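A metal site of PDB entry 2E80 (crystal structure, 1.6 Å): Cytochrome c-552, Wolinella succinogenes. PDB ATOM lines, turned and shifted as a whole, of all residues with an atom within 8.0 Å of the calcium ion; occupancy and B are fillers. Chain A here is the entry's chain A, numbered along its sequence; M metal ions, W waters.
The calcium ion is bound by the side-chain amide oxygen (OE1) of Gln 254, at 2.3 Å. The calcium ion is bound by O of Lys 252, at 2.3 Å. The calcium ion is bound by O of Tyr 196. The side-chain carboxylate (OE2) of Glu 195 binds the calcium ion. Water W2 is bound to the calcium ion (2.5 Å). Water W1 is bound to the calcium ion (2.5 Å). The side-chain carboxylate (OE1) of Glu 195 binds the calcium ion (2.6 Å).
Residues that only touch the calcium ion: Tyr 233 (3.9 Å). The nearest printed residue that does not touch the calcium ion is Ala 253 (4.2 Å).
Water W2 lies within hydrogen-bond range of OD2 of Asp 240 (2.7 Å) and OH of Tyr 233 (3.1 Å). Water W1 bridges OD1 of Asp 240 and NE2 of Gln 254.
OE2 of Glu 195 sits close to OH of Tyr 233 (2.5 Å). The side-chain carboxylate (OD2) of Asp 372 lies within salt-bridge range of the side-chain amino group (NZ) of Lys 252, at 2.9 Å. The backbone carbonyl oxygen (O) of Tyr 233 lies within hydrogen-bond range of the backbone NH (N) of Phe 238 (2.9 Å). The backbone NH of Lys 252 is in hydrogen-bond range of the side-chain carboxylate of Asp 240 (2.7 Å).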
ATOM      1  N   TYR A  68     -19.133   0.778   6.267  1.00  0.00           N
ATOM      2  CA  TYR A  68     -19.824   1.587   7.262  1.00  0.00           C
ATOM      3  C   TYR A  68     -19.317   3.026   7.153  1.00  0.00           C
ATOM      4  O   TYR A  68     -18.175   3.256   6.744  1.00  0.00           O
ATOM      5  CB  TYR A  68     -19.541   1.020   8.671  1.00  0.00           C
ATOM      6  CG  TYR A  68     -20.572   1.359   9.719  1.00  0.00           C
ATOM      7  CD1 TYR A  68     -21.919   1.046   9.526  1.00  0.00           C
ATOM      8  CD2 TYR A  68     -20.197   1.957  10.915  1.00  0.00           C
ATOM      9  CE1 TYR A  68     -22.869   1.332  10.517  1.00  0.00           C
ATOM     10  CE2 TYR A  68     -21.133   2.244  11.906  1.00  0.00           C
ATOM     11  CZ  TYR A  68     -22.473   1.925  11.692  1.00  0.00           C
ATOM     12  OH  TYR A  68     -23.402   2.211  12.671  1.00  0.00           O
ATOM     13  N   VAL A 194     -22.047   7.490  26.186  1.00  0.00           N
ATOM     14  CA  VAL A 194     -22.365   6.073  26.373  1.00  0.00           C
ATOM     15  C   VAL A 194     -22.523   5.386  25.012  1.00  0.00           C
ATOM     16  O   VAL A 194     -22.642   6.041  23.984  1.00  0.00           O
ATOM     17  CB  VAL A 194     -23.695   5.908  27.145  1.00  0.00           C
ATOM     18  CG1 VAL A 194     -23.545   6.384  28.582  1.00  0.00           C
ATOM     19  CG2 VAL A 194     -24.797   6.688  26.446  1.00  0.00           C
ATOM     20  N   GLU A 195     -22.523   4.057  25.038  1.00  0.00           N
ATOM     21  CA  GLU A 195     -22.715   3.249  23.834  1.00  0.00           C
ATOM     22  C   GLU A 195     -24.224   3.165  23.571  1.00  0.00           C
ATOM     23  O   GLU A 195     -25.022   3.124  24.505  1.00  0.00           O
ATOM     24  CB  GLU A 195     -22.127   1.845  24.053  1.00  0.00           C
ATOM     25  CG  GLU A 195     -22.877   0.677  23.394  1.00  0.00           C
ATOM     26  CD  GLU A 195     -22.873   0.710  21.867  1.00  0.00           C
ATOM     27  OE1 GLU A 195     -22.123   1.507  21.266  1.00  0.00           O
ATOM     28  OE2 GLU A 195     -23.629  -0.090  21.275  1.00  0.00           O
ATOM     29  N   TYR A 196     -24.603   3.153  22.296  1.00  0.00           N
ATOM     30  CA  TYR A 196     -26.007   3.113  21.938  1.00  0.00           C
ATOM     31  C   TYR A 196     -26.208   2.431  20.584  1.00  0.00           C
ATOM     32  O   TYR A 196     -25.251   2.102  19.895  1.00  0.00           O
ATOM     33  CB  TYR A 196     -26.554   4.542  21.816  1.00  0.00           C
ATOM     34  CG  TYR A 196     -26.071   5.233  20.551  1.00  0.00           C
ATOM     35  CD1 TYR A 196     -24.800   5.795  20.469  1.00  0.00           C
ATOM     36  CD2 TYR A 196     -26.853   5.202  19.393  1.00  0.00           C
ATOM     37  CE1 TYR A 196     -24.320   6.322  19.258  1.00  0.00           C
ATOM     38  CE2 TYR A 196     -26.379   5.711  18.194  1.00  0.00           C
ATOM     39  CZ  TYR A 196     -25.123   6.268  18.129  1.00  0.00           C
ATOM     40  OH  TYR A 196     -24.662   6.754  16.923  1.00  0.00           O
ATOM     41  N   TYR A 197     -27.472   2.223  20.223  1.00  0.00           N
ATOM     42  CA  TYR A 197     -27.820   1.694  18.910  1.00  0.00           C
ATOM     43  C   TYR A 197     -29.180   2.264  18.558  1.00  0.00           C
ATOM     44  O   TYR A 197     -29.935   2.655  19.447  1.00  0.00           O
ATOM     45  CB  TYR A 197     -27.856   0.148  18.890  1.00  0.00           C
ATOM     46  CG  TYR A 197     -29.091  -0.521  19.464  1.00  0.00           C
ATOM     47  CD1 TYR A 197     -29.207  -0.762  20.832  1.00  0.00           C
ATOM     48  CD2 TYR A 197     -30.118  -0.955  18.625  1.00  0.00           C
ATOM     49  CE1 TYR A 197     -30.315  -1.436  21.350  1.00  0.00           C
ATOM     50  CE2 TYR A 197     -31.225  -1.635  19.136  1.00  0.00           C
ATOM     51  CZ  TYR A 197     -31.320  -1.869  20.500  1.00  0.00           C
ATOM     52  OH  TYR A 197     -32.391  -2.566  20.999  1.00  0.00           O
ATOM     53  N   PHE A 198     -29.477   2.363  17.263  1.00  0.00           N
ATOM     54  CA  PHE A 198     -30.771   2.895  16.827  1.00  0.00           C
ATOM     55  C   PHE A 198     -31.760   1.747  16.692  1.00  0.00           C
ATOM     56  O   PHE A 198     -31.533   0.813  15.919  1.00  0.00           O
ATOM     57  CB  PHE A 198     -30.649   3.606  15.472  1.00  0.00           C
ATOM     58  CG  PHE A 198     -29.841   4.870  15.498  1.00  0.00           C
ATOM     59  CD1 PHE A 198     -29.761   5.643  16.662  1.00  0.00           C
ATOM     60  CD2 PHE A 198     -29.188   5.313  14.358  1.00  0.00           C
ATOM     61  CE1 PHE A 198     -29.042   6.840  16.661  1.00  0.00           C
ATOM     62  CE2 PHE A 198     -28.469   6.504  14.349  1.00  0.00           C
ATOM     63  CZ  PHE A 198     -28.403   7.270  15.505  1.00  0.00           C
ATOM     64  N   THR A 217     -31.152   3.880  21.778  1.00  0.00           N
ATOM     65  CA  THR A 217     -31.362   2.885  22.819  1.00  0.00           C
ATOM     66  C   THR A 217     -30.037   2.443  23.426  1.00  0.00           C
ATOM     67  O   THR A 217     -29.081   2.154  22.718  1.00  0.00           O
ATOM     68  CB  THR A 217     -32.061   1.647  22.217  1.00  0.00           C
ATOM     69  OG1 THR A 217     -33.264   2.045  21.560  1.00  0.00           O
ATOM     70  CG2 THR A 217     -32.384   0.640  23.315  1.00  0.00           C
ATOM     71  N   PRO A 219     -27.980  -0.347  25.074  1.00  0.00           N
ATOM     72  CA  PRO A 219     -27.969  -1.811  25.168  1.00  0.00           C
ATOM     73  C   PRO A 219     -27.567  -2.318  26.546  1.00  0.00           C
ATOM     74  O   PRO A 219     -26.658  -3.139  26.674  1.00  0.00           O
ATOM     75  CB  PRO A 219     -26.965  -2.204  24.097  1.00  0.00           C
ATOM     76  CG  PRO A 219     -25.925  -1.122  24.249  1.00  0.00           C
ATOM     77  CD  PRO A 219     -26.780   0.134  24.353  1.00  0.00           C
ATOM     78  N   MET A 229     -23.401  -6.608  26.973  1.00  0.00           N
ATOM     79  CA  MET A 229     -23.946  -5.890  25.832  1.00  0.00           C
ATOM     80  C   MET A 229     -23.837  -6.788  24.594  1.00  0.00           C
ATOM     81  O   MET A 229     -24.715  -6.778  23.731  1.00  0.00           O
ATOM     82  CB  MET A 229     -23.179  -4.588  25.610  1.00  0.00           C
ATOM     83  CG  MET A 229     -23.497  -3.521  26.645  1.00  0.00           C
ATOM     84  SD  MET A 229     -22.752  -1.924  26.203  1.00  0.00           S
ATOM     85  CE  MET A 229     -21.878  -1.527  27.675  1.00  0.00           C
ATOM     86  N   TYR A 233     -26.945  -7.877  22.041  1.00  0.00           N
ATOM     87  CA  TYR A 233     -27.001  -7.784  20.593  1.00  0.00           C
ATOM     88  C   TYR A 233     -27.158  -9.126  19.886  1.00  0.00           C
ATOM     89  O   TYR A 233     -27.861  -9.222  18.883  1.00  0.00           O
ATOM     90  CB  TYR A 233     -25.753  -7.060  20.065  1.00  0.00           C
ATOM     91  CG  TYR A 233     -25.753  -5.571  20.346  1.00  0.00           C
ATOM     92  CD1 TYR A 233     -26.787  -4.766  19.883  1.00  0.00           C
ATOM     93  CD2 TYR A 233     -24.717  -4.971  21.053  1.00  0.00           C
ATOM     94  CE1 TYR A 233     -26.797  -3.395  20.104  1.00  0.00           C
ATOM     95  CE2 TYR A 233     -24.706  -3.593  21.294  1.00  0.00           C
ATOM     96  CZ  TYR A 233     -25.760  -2.812  20.812  1.00  0.00           C
ATOM     97  OH  TYR A 233     -25.770  -1.448  21.025  1.00  0.00           O
ATOM     98  N   PHE A 238     -28.885  -8.627  16.207  1.00  0.00           N
ATOM     99  CA  PHE A 238     -28.648  -7.286  15.696  1.00  0.00           C
ATOM    100  C   PHE A 238     -27.298  -7.104  15.025  1.00  0.00           C
ATOM    101  O   PHE A 238     -26.312  -7.712  15.420  1.00  0.00           O
ATOM    102  CB  PHE A 238     -28.760  -6.277  16.846  1.00  0.00           C
ATOM    103  CG  PHE A 238     -28.675  -4.845  16.398  1.00  0.00           C
ATOM    104  CD1 PHE A 238     -29.781  -4.202  15.857  1.00  0.00           C
ATOM    105  CD2 PHE A 238     -27.474  -4.149  16.501  1.00  0.00           C
ATOM    106  CE1 PHE A 238     -29.706  -2.885  15.424  1.00  0.00           C
ATOM    107  CE2 PHE A 238     -27.385  -2.821  16.059  1.00  0.00           C
ATOM    108  CZ  PHE A 238     -28.498  -2.194  15.531  1.00  0.00           C
ATOM    109  N   ASP A 240     -25.114  -3.679  13.107  1.00  0.00           N
ATOM    110  CA  ASP A 240     -25.112  -2.290  12.677  1.00  0.00           C
ATOM    111  C   ASP A 240     -24.904  -2.233  11.164  1.00  0.00           C
ATOM    112  O   ASP A 240     -25.436  -1.358  10.485  1.00  0.00           O
ATOM    113  CB  ASP A 240     -24.032  -1.507  13.420  1.00  0.00           C
ATOM    114  CG  ASP A 240     -24.413  -1.238  14.863  1.00  0.00           C
ATOM    115  OD1 ASP A 240     -25.359  -0.458  15.084  1.00  0.00           O
ATOM    116  OD2 ASP A 240     -23.779  -1.819  15.773  1.00  0.00           O
ATOM    117  N   LEU A 251     -21.004  -5.158  14.708  1.00  0.00           N
ATOM    118  CA  LEU A 251     -21.506  -4.321  15.789  1.00  0.00           C
ATOM    119  C   LEU A 251     -20.540  -3.154  15.960  1.00  0.00           C
ATOM    120  O   LEU A 251     -19.324  -3.356  16.018  1.00  0.00           O
ATOM    121  CB  LEU A 251     -21.583  -5.095  17.107  1.00  0.00           C
ATOM    122  CG  LEU A 251     -22.595  -6.226  17.211  1.00  0.00           C
ATOM    123  CD1 LEU A 251     -22.354  -6.999  18.487  1.00  0.00           C
ATOM    124  CD2 LEU A 251     -24.000  -5.653  17.186  1.00  0.00           C
ATOM    125  N   LYS A 252     -21.081  -1.948  16.013  1.00  0.00           N
ATOM    126  CA  LYS A 252     -20.272  -0.739  16.197  1.00  0.00           C
ATOM    127  C   LYS A 252     -20.384  -0.219  17.616  1.00  0.00           C
ATOM    128  O   LYS A 252     -21.479   0.054  18.103  1.00  0.00           O
ATOM    129  CB  LYS A 252     -20.739   0.372  15.245  1.00  0.00           C
ATOM    130  CG  LYS A 252     -19.888   1.641  15.320  1.00  0.00           C
ATOM    131  CD  LYS A 252     -18.547   1.467  14.597  1.00  0.00           C
ATOM    132  CE  LYS A 252     -17.596   2.622  14.891  1.00  0.00           C
ATOM    133  NZ  LYS A 252     -17.009   2.531  16.267  1.00  0.00           N
ATOM    134  N   ALA A 253     -19.255  -0.069  18.286  1.00  0.00           N
ATOM    135  CA  ALA A 253     -19.247   0.462  19.637  1.00  0.00           C
ATOM    136  C   ALA A 253     -19.025   1.966  19.506  1.00  0.00           C
ATOM    137  O   ALA A 253     -18.233   2.400  18.670  1.00  0.00           O
ATOM    138  CB  ALA A 253     -18.130  -0.167  20.447  1.00  0.00           C
ATOM    139  N   GLN A 254     -19.728   2.748  20.306  1.00  0.00           N
ATOM    140  CA  GLN A 254     -19.548   4.187  20.276  1.00  0.00           C
ATOM    141  C   GLN A 254     -19.307   4.716  21.674  1.00  0.00           C
ATOM    142  O   GLN A 254     -20.135   4.521  22.563  1.00  0.00           O
ATOM    143  CB  GLN A 254     -20.748   4.916  19.652  1.00  0.00           C
ATOM    144  CG  GLN A 254     -20.892   4.714  18.152  1.00  0.00           C
ATOM    145  CD  GLN A 254     -22.005   3.753  17.814  1.00  0.00           C
ATOM    146  OE1 GLN A 254     -22.367   2.910  18.630  1.00  0.00           O
ATOM    147  NE2 GLN A 254     -22.544   3.860  16.606  1.00  0.00           N
ATOM    148  N   HIS A 255     -18.161   5.352  21.862  1.00  0.00           N
ATOM    149  CA  HIS A 255     -17.773   5.988  23.104  1.00  0.00           C
ATOM    150  C   HIS A 255     -18.526   5.542  24.358  1.00  0.00           C
ATOM    151  O   HIS A 255     -19.388   6.264  24.870  1.00  0.00           O
ATOM    152  CB  HIS A 255     -17.933   7.496  22.945  1.00  0.00           C
ATOM    153  CG  HIS A 255     -19.207   7.884  22.256  1.00  0.00           C
ATOM    154  ND1 HIS A 255     -20.441   7.618  22.793  1.00  0.00           N
ATOM    155  CD2 HIS A 255     -19.427   8.434  21.040  1.00  0.00           C
ATOM    156  CE1 HIS A 255     -21.380   8.002  21.939  1.00  0.00           C
ATOM    157  NE2 HIS A 255     -20.786   8.498  20.869  1.00  0.00           N
ATOM    158  N   TRP A 369     -16.143  -6.269  18.308  1.00  0.00           N
ATOM    159  CA  TRP A 369     -17.019  -5.645  19.290  1.00  0.00           C
ATOM    160  C   TRP A 369     -16.232  -5.348  20.558  1.00  0.00           C
ATOM    161  O   TRP A 369     -16.300  -4.252  21.107  1.00  0.00           O
ATOM    162  CB  TRP A 369     -18.203  -6.561  19.640  1.00  0.00           C
ATOM    163  CG  TRP A 369     -18.978  -6.063  20.826  1.00  0.00           C
ATOM    164  CD1 TRP A 369     -19.074  -6.657  22.053  1.00  0.00           C
ATOM    165  CD2 TRP A 369     -19.704  -4.825  20.925  1.00  0.00           C
ATOM    166  NE1 TRP A 369     -19.827  -5.880  22.906  1.00  0.00           N
ATOM    167  CE2 TRP A 369     -20.226  -4.747  22.232  1.00  0.00           C
ATOM    168  CE3 TRP A 369     -19.978  -3.786  20.024  1.00  0.00           C
ATOM    169  CZ2 TRP A 369     -20.993  -3.661  22.665  1.00  0.00           C
ATOM    170  CZ3 TRP A 369     -20.744  -2.712  20.465  1.00  0.00           C
ATOM    171  CH2 TRP A 369     -21.244  -2.662  21.770  1.00  0.00           C
ATOM    172  N   ASP A 372     -13.383  -2.674  19.837  1.00  0.00           N
ATOM    173  CA  ASP A 372     -13.960  -1.358  19.585  1.00  0.00           C
ATOM    174  C   ASP A 372     -14.463  -0.786  20.913  1.00  0.00           C
ATOM    175  O   ASP A 372     -14.270   0.398  21.211  1.00  0.00           O
ATOM    176  CB  ASP A 372     -15.117  -1.468  18.579  1.00  0.00           C
ATOM    177  CG  ASP A 372     -15.372  -0.167  17.828  1.00  0.00           C
ATOM    178  OD1 ASP A 372     -14.619   0.816  18.035  1.00  0.00           O
ATOM    179  OD2 ASP A 372     -16.328  -0.139  17.025  1.00  0.00           O
ATOM    180  N   MET A 373     -15.107  -1.627  21.718  1.00  0.00           N
ATOM    181  CA  MET A 373     -15.599  -1.172  23.023  1.00  0.00           C
ATOM    182  C   MET A 373     -14.447  -0.675  23.892  1.00  0.00           C
ATOM    183  O   MET A 373     -14.616   0.223  24.708  1.00  0.00           O
ATOM    184  CB  MET A 373     -16.326  -2.303  23.748  1.00  0.00           C
ATOM    185  CG  MET A 373     -17.805  -2.413  23.404  1.00  0.00           C
ATOM    186  SD  MET A 373     -18.753  -1.006  24.024  1.00  0.00           S
ATOM    187  CE  MET A 373     -18.693  -1.309  25.777  1.00  0.00           C
HETATM  188 CA    CA M   1     -23.390   0.940  19.075  1.00  0.00          CA
HETATM  189  O   HOH W   1     -24.486   1.458  16.852  1.00  0.00           O
HETATM  190  O   HOH W   2     -24.312  -1.255  18.339  1.00  0.00           O
